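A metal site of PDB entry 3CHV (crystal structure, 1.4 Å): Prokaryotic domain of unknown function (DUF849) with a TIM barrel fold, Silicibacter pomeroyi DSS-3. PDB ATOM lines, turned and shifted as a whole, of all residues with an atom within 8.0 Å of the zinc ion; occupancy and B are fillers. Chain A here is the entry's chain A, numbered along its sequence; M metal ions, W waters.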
ATOM      1  N   ALA A  15       8.842  20.205 -16.390  1.00  0.00           N
ATOM      2  CA  ALA A  15      10.085  19.680 -16.920  1.00  0.00           C
ATOM      3  C   ALA A  15      10.363  20.444 -18.238  1.00  0.00           C
ATOM      4  O   ALA A  15       9.797  20.172 -19.289  1.00  0.00           O
ATOM      5  CB  ALA A  15       9.970  18.167 -17.127  1.00  0.00           C
ATOM      6  N   ILE A  16      11.140  21.483 -18.079  1.00  0.00           N
ATOM      7  CA  ILE A  16      11.196  22.584 -19.072  1.00  0.00           C
ATOM      8  C   ILE A  16      11.948  22.315 -20.371  1.00  0.00           C
ATOM      9  O   ILE A  16      11.583  22.850 -21.413  1.00  0.00           O
ATOM     10  CB  ILE A  16      11.762  23.895 -18.437  1.00  0.00           C
ATOM     11  CG1 ILE A  16      13.156  23.689 -17.860  1.00  0.00           C
ATOM     12  CG2 ILE A  16      10.829  24.441 -17.332  1.00  0.00           C
ATOM     13  CD1 ILE A  16      13.908  25.024 -17.562  1.00  0.00           C
ATOM     14  N   THR A  17      12.959  21.466 -20.321  1.00  0.00           N
ATOM     15  CA  THR A  17      13.956  21.363 -21.424  1.00  0.00           C
ATOM     16  C   THR A  17      14.381  19.935 -21.718  1.00  0.00           C
ATOM     17  O   THR A  17      14.361  19.471 -22.850  1.00  0.00           O
ATOM     18  CB  THR A  17      15.212  22.220 -21.104  1.00  0.00           C
ATOM     19  OG1 THR A  17      14.794  23.586 -21.008  1.00  0.00           O
ATOM     20  CG2 THR A  17      16.265  22.092 -22.188  1.00  0.00           C
ATOM     21  N   GLY A  18      14.813  19.221 -20.684  1.00  0.00           N
ATOM     22  CA  GLY A  18      15.301  17.859 -20.903  1.00  0.00           C
ATOM     23  C   GLY A  18      16.632  17.826 -21.591  1.00  0.00           C
ATOM     24  O   GLY A  18      17.339  18.830 -21.670  1.00  0.00           O
ATOM     25  N   SER A  19      16.963  16.649 -22.120  1.00  0.00           N
ATOM     26  CA  SER A  19      18.215  16.494 -22.899  1.00  0.00           C
ATOM     27  C   SER A  19      17.997  16.304 -24.373  1.00  0.00           C
ATOM     28  O   SER A  19      18.884  16.606 -25.167  1.00  0.00           O
ATOM     29  CB  SER A  19      19.088  15.313 -22.390  1.00  0.00           C
ATOM     30  OG  SER A  19      18.365  14.098 -22.505  1.00  0.00           O
ATOM     31  N   HIS A  52      11.851  21.191 -12.969  1.00  0.00           N
ATOM     32  CA  HIS A  52      12.789  20.087 -13.219  1.00  0.00           C
ATOM     33  C   HIS A  52      13.693  20.498 -14.373  1.00  0.00           C
ATOM     34  O   HIS A  52      13.226  20.711 -15.501  1.00  0.00           O
ATOM     35  CB  HIS A  52      12.022  18.805 -13.503  1.00  0.00           C
ATOM     36  CG  HIS A  52      12.872  17.686 -14.028  1.00  0.00           C
ATOM     37  ND1 HIS A  52      13.592  16.834 -13.219  1.00  0.00           N
ATOM     38  CD2 HIS A  52      13.159  17.330 -15.296  1.00  0.00           C
ATOM     39  CE1 HIS A  52      14.261  15.983 -13.969  1.00  0.00           C
ATOM     40  NE2 HIS A  52      14.035  16.276 -15.247  1.00  0.00           N
ATOM     41  N   CYS A  53      14.950  20.684 -14.038  1.00  0.00           N
ATOM     42  CA  CYS A  53      15.920  21.392 -14.883  1.00  0.00           C
ATOM     43  C   CYS A  53      17.045  20.515 -15.395  1.00  0.00           C
ATOM     44  O   CYS A  53      17.653  19.754 -14.679  1.00  0.00           O
ATOM     45  CB  CYS A  53      16.615  22.501 -14.061  1.00  0.00           C
ATOM     46  SG  CYS A  53      15.466  23.732 -13.404  1.00  0.00           S
ATOM     47  N   HIS A  54      17.319  20.700 -16.691  1.00  0.00           N
ATOM     48  CA  HIS A  54      18.544  20.320 -17.380  1.00  0.00           C
ATOM     49  C   HIS A  54      19.084  21.592 -17.971  1.00  0.00           C
ATOM     50  O   HIS A  54      18.371  22.587 -18.132  1.00  0.00           O
ATOM     51  CB  HIS A  54      18.269  19.367 -18.545  1.00  0.00           C
ATOM     52  CG  HIS A  54      17.645  18.049 -18.180  1.00  0.00           C
ATOM     53  ND1 HIS A  54      18.217  16.843 -18.516  1.00  0.00           N
ATOM     54  CD2 HIS A  54      16.451  17.760 -17.614  1.00  0.00           C
ATOM     55  CE1 HIS A  54      17.411  15.870 -18.101  1.00  0.00           C
ATOM     56  NE2 HIS A  54      16.328  16.401 -17.578  1.00  0.00           N
ATOM     57  N   GLN A  86      14.739  21.794  -8.964  1.00  0.00           N
ATOM     58  CA  GLN A  86      15.134  20.372  -9.010  1.00  0.00           C
ATOM     59  C   GLN A  86      16.066  20.149 -10.171  1.00  0.00           C
ATOM     60  O   GLN A  86      15.729  20.402 -11.312  1.00  0.00           O
ATOM     61  CB  GLN A  86      13.905  19.496  -9.142  1.00  0.00           C
ATOM     62  CG  GLN A  86      14.183  18.019  -9.206  1.00  0.00           C
ATOM     63  CD  GLN A  86      12.962  17.211  -9.496  1.00  0.00           C
ATOM     64  OE1 GLN A  86      12.798  16.746 -10.603  1.00  0.00           O
ATOM     65  NE2 GLN A  86      12.072  17.065  -8.499  1.00  0.00           N
ATOM     66  N   PHE A  87      17.264  19.729  -9.855  1.00  0.00           N
ATOM     67  CA  PHE A  87      18.244  19.421 -10.886  1.00  0.00           C
ATOM     68  C   PHE A  87      18.145  17.985 -11.363  1.00  0.00           C
ATOM     69  O   PHE A  87      17.973  17.058 -10.590  1.00  0.00           O
ATOM     70  CB  PHE A  87      19.676  19.590 -10.351  1.00  0.00           C
ATOM     71  CG  PHE A  87      20.098  21.000 -10.013  1.00  0.00           C
ATOM     72  CD1 PHE A  87      19.361  22.102 -10.367  1.00  0.00           C
ATOM     73  CD2 PHE A  87      21.298  21.175  -9.397  1.00  0.00           C
ATOM     74  CE1 PHE A  87      19.820  23.386 -10.031  1.00  0.00           C
ATOM     75  CE2 PHE A  87      21.802  22.427  -9.126  1.00  0.00           C
ATOM     76  CZ  PHE A  87      21.088  23.533  -9.450  1.00  0.00           C
ATOM     77  N   SER A  88      18.309  17.781 -12.665  1.00  0.00           N
ATOM     78  CA  SER A  88      18.504  16.416 -13.246  1.00  0.00           C
ATOM     79  C   SER A  88      19.923  15.897 -12.949  1.00  0.00           C
ATOM     80  O   SER A  88      20.871  16.680 -12.932  1.00  0.00           O
ATOM     81  CB  SER A  88      18.304  16.508 -14.774  1.00  0.00           C
ATOM     82  OG  SER A  88      18.546  15.252 -15.400  1.00  0.00           O
ATOM     83  N   THR A  89      20.071  14.569 -12.748  1.00  0.00           N
ATOM     84  CA  THR A  89      21.346  13.851 -12.711  1.00  0.00           C
ATOM     85  C   THR A  89      21.354  12.836 -13.863  1.00  0.00           C
ATOM     86  O   THR A  89      21.947  11.772 -13.759  1.00  0.00           O
ATOM     87  CB  THR A  89      21.572  13.115 -11.363  1.00  0.00           C
ATOM     88  OG1 THR A  89      20.538  12.154 -11.117  1.00  0.00           O
ATOM     89  CG2 THR A  89      21.593  14.153 -10.237  1.00  0.00           C
ATOM     90  N   GLY A  90      20.694  13.252 -14.931  1.00  0.00           N
ATOM     91  CA  GLY A  90      20.424  12.432 -16.072  1.00  0.00           C
ATOM     92  C   GLY A  90      21.584  12.002 -16.810  1.00  0.00           C
ATOM     93  O   GLY A  90      22.611  12.698 -16.964  1.00  0.00           O
ATOM     94  N   SER A  93      22.282  13.509 -20.175  1.00  0.00           N
ATOM     95  CA  SER A  93      22.886  14.889 -20.054  1.00  0.00           C
ATOM     96  C   SER A  93      24.366  14.880 -19.650  1.00  0.00           C
ATOM     97  O   SER A  93      25.124  15.856 -19.888  1.00  0.00           O
ATOM     98  CB  SER A  93      22.091  15.727 -19.055  1.00  0.00           C
ATOM     99  OG  SER A  93      20.858  16.235 -19.545  1.00  0.00           O
ATOM    100  N   SER A 111      16.553  14.948  -9.321  1.00  0.00           N
ATOM    101  CA  SER A 111      15.996  13.676  -9.782  1.00  0.00           C
ATOM    102  C   SER A 111      17.103  12.618  -9.711  1.00  0.00           C
ATOM    103  O   SER A 111      18.263  12.925  -9.948  1.00  0.00           O
ATOM    104  CB  SER A 111      15.360  13.803 -11.174  1.00  0.00           C
ATOM    105  OG  SER A 111      16.312  14.191 -12.142  1.00  0.00           O
ATOM    106  N   TYR A 124      19.552   2.806 -20.493  1.00  0.00           N
ATOM    107  CA  TYR A 124      19.694   3.947 -19.555  1.00  0.00           C
ATOM    108  C   TYR A 124      20.430   3.392 -18.321  1.00  0.00           C
ATOM    109  O   TYR A 124      19.851   2.726 -17.441  1.00  0.00           O
ATOM    110  CB  TYR A 124      18.338   4.544 -19.206  1.00  0.00           C
ATOM    111  CG  TYR A 124      18.482   5.800 -18.447  1.00  0.00           C
ATOM    112  CD1 TYR A 124      19.319   6.794 -18.913  1.00  0.00           C
ATOM    113  CD2 TYR A 124      17.747   6.038 -17.309  1.00  0.00           C
ATOM    114  CE1 TYR A 124      19.503   7.966 -18.176  1.00  0.00           C
ATOM    115  CE2 TYR A 124      17.855   7.236 -16.612  1.00  0.00           C
ATOM    116  CZ  TYR A 124      18.720   8.182 -17.034  1.00  0.00           C
ATOM    117  OH  TYR A 124      18.871   9.372 -16.342  1.00  0.00           O
ATOM    118  N   GLU A 148      13.132   8.693  -9.998  1.00  0.00           N
ATOM    119  CA  GLU A 148      12.553   8.536 -11.315  1.00  0.00           C
ATOM    120  C   GLU A 148      12.451   7.046 -11.557  1.00  0.00           C
ATOM    121  O   GLU A 148      13.430   6.387 -11.942  1.00  0.00           O
ATOM    122  CB  GLU A 148      13.475   9.151 -12.347  1.00  0.00           C
ATOM    123  CG  GLU A 148      13.750  10.641 -12.034  1.00  0.00           C
ATOM    124  CD  GLU A 148      12.443  11.409 -11.933  1.00  0.00           C
ATOM    125  OE1 GLU A 148      11.496  11.127 -12.660  1.00  0.00           O
ATOM    126  OE2 GLU A 148      12.383  12.314 -11.070  1.00  0.00           O
ATOM    127  N   PHE A 150      11.337   4.005 -13.500  1.00  0.00           N
ATOM    128  CA  PHE A 150      11.021   3.594 -14.867  1.00  0.00           C
ATOM    129  C   PHE A 150      10.457   2.173 -14.941  1.00  0.00           C
ATOM    130  O   PHE A 150      10.078   1.678 -15.996  1.00  0.00           O
ATOM    131  CB  PHE A 150      12.217   3.731 -15.768  1.00  0.00           C
ATOM    132  CG  PHE A 150      12.617   5.173 -16.055  1.00  0.00           C
ATOM    133  CD1 PHE A 150      12.120   5.857 -17.127  1.00  0.00           C
ATOM    134  CD2 PHE A 150      13.528   5.805 -15.216  1.00  0.00           C
ATOM    135  CE1 PHE A 150      12.516   7.170 -17.353  1.00  0.00           C
ATOM    136  CE2 PHE A 150      13.926   7.136 -15.456  1.00  0.00           C
ATOM    137  CZ  PHE A 150      13.430   7.767 -16.551  1.00  0.00           C
ATOM    138  N   GLN A 174       8.487   9.262  -8.454  1.00  0.00           N
ATOM    139  CA  GLN A 174       7.814   9.555  -9.721  1.00  0.00           C
ATOM    140  C   GLN A 174       7.714   8.335 -10.596  1.00  0.00           C
ATOM    141  O   GLN A 174       8.728   7.714 -10.930  1.00  0.00           O
ATOM    142  CB  GLN A 174       8.478  10.667 -10.491  1.00  0.00           C
ATOM    143  CG  GLN A 174       7.671  11.010 -11.762  1.00  0.00           C
ATOM    144  CD  GLN A 174       8.002  12.302 -12.290  1.00  0.00           C
ATOM    145  OE1 GLN A 174       7.225  13.270 -12.169  1.00  0.00           O
ATOM    146  NE2 GLN A 174       9.200  12.377 -12.872  1.00  0.00           N
ATOM    147  N   ARG A 230       3.620  15.802 -13.283  1.00  0.00           N
ATOM    148  CA  ARG A 230       4.613  16.553 -14.077  1.00  0.00           C
ATOM    149  C   ARG A 230       4.111  16.732 -15.467  1.00  0.00           C
ATOM    150  O   ARG A 230       3.345  15.937 -16.011  1.00  0.00           O
ATOM    151  CB  ARG A 230       5.959  15.784 -14.110  1.00  0.00           C
ATOM    152  CG  ARG A 230       7.063  16.396 -14.864  1.00  0.00           C
ATOM    153  CD  ARG A 230       8.355  15.648 -14.590  1.00  0.00           C
ATOM    154  NE  ARG A 230       8.993  15.128 -15.756  1.00  0.00           N
ATOM    155  CZ  ARG A 230      10.215  14.676 -15.744  1.00  0.00           C
ATOM    156  NH1 ARG A 230      10.897  14.572 -14.626  1.00  0.00           N
ATOM    157  NH2 ARG A 230      10.753  14.237 -16.870  1.00  0.00           N
ATOM    158  N   GLU A 234      10.073  18.826 -22.032  1.00  0.00           N
ATOM    159  CA  GLU A 234      10.971  17.704 -21.885  1.00  0.00           C
ATOM    160  C   GLU A 234      10.299  16.423 -22.257  1.00  0.00           C
ATOM    161  O   GLU A 234      10.842  15.508 -22.836  1.00  0.00           O
ATOM    162  CB  GLU A 234      11.494  17.614 -20.453  1.00  0.00           C
ATOM    163  CG  GLU A 234      12.235  16.312 -20.191  1.00  0.00           C
ATOM    164  CD  GLU A 234      13.037  16.347 -18.927  1.00  0.00           C
ATOM    165  OE1 GLU A 234      13.285  17.403 -18.336  1.00  0.00           O
ATOM    166  OE2 GLU A 234      13.496  15.234 -18.506  1.00  0.00           O
ATOM    167  N   ASP A 235       9.073  16.284 -21.773  1.00  0.00           N
ATOM    168  CA  ASP A 235       8.320  15.020 -21.881  1.00  0.00           C
ATOM    169  C   ASP A 235       7.403  14.871 -23.079  1.00  0.00           C
ATOM    170  O   ASP A 235       7.097  13.797 -23.499  1.00  0.00           O
ATOM    171  CB  ASP A 235       7.497  14.738 -20.629  1.00  0.00           C
ATOM    172  CG  ASP A 235       8.341  14.563 -19.343  1.00  0.00           C
ATOM    173  OD1 ASP A 235       9.525  14.181 -19.414  1.00  0.00           O
ATOM    174  OD2 ASP A 235       7.753  14.837 -18.257  1.00  0.00           O
HETATM  175 ZN    ZN M   1      14.712  15.350 -16.947  1.00  0.00          ZN
HETATM  176  O   HOH W   1      13.478  13.165 -15.693  1.00  0.00           O
HETATM  177  O   HOH W   2      15.046  13.414 -17.264  1.00  0.00           O
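The zinc ion is bound by the side-chain carboxylate (OE2) of Glu 234 (2.0 Å).
Water W2 binds the zinc ion (2.0 Å).
A ring nitrogen (NE2) of His 54 binds the zinc ion, at 2.0 Å.
The zinc ion is bound by a ring nitrogen (NE2) of His 52 (2.1 Å).
The zinc ion has four donor atoms within binding distance.
Slightly farther from the zinc ion lies water W1 (2.8 Å).
The side-chain carboxylate of Glu 234 lies close to the guanidinium group of Arg 230 (3.3 Å).
OE1 of Glu 234 lies close to N of Gly 18, at 3.3 Å.
The backbone NH of Glu 234 lies within hydrogen-bond range of the backbone carbonyl oxygen of Ala 15 (3.1 Å).
A ring nitrogen (NE2) of His 54 lies close to the side-chain hydroxyl (OG) of Ser 88, 3.3 Å away.
ND1 of His 54 lies within hydrogen-bond range of OG of Ser 93 (2.9 Å).
A ring nitrogen (ND1) of His 52 sits at hydrogen-bond distance from the side-chain amide oxygen of Gln 86 (2.7 Å).
The backbone carbonyl oxygen of His 52 lies within hydrogen-bond range of the backbone NH of Ile 16 (3.4 Å).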
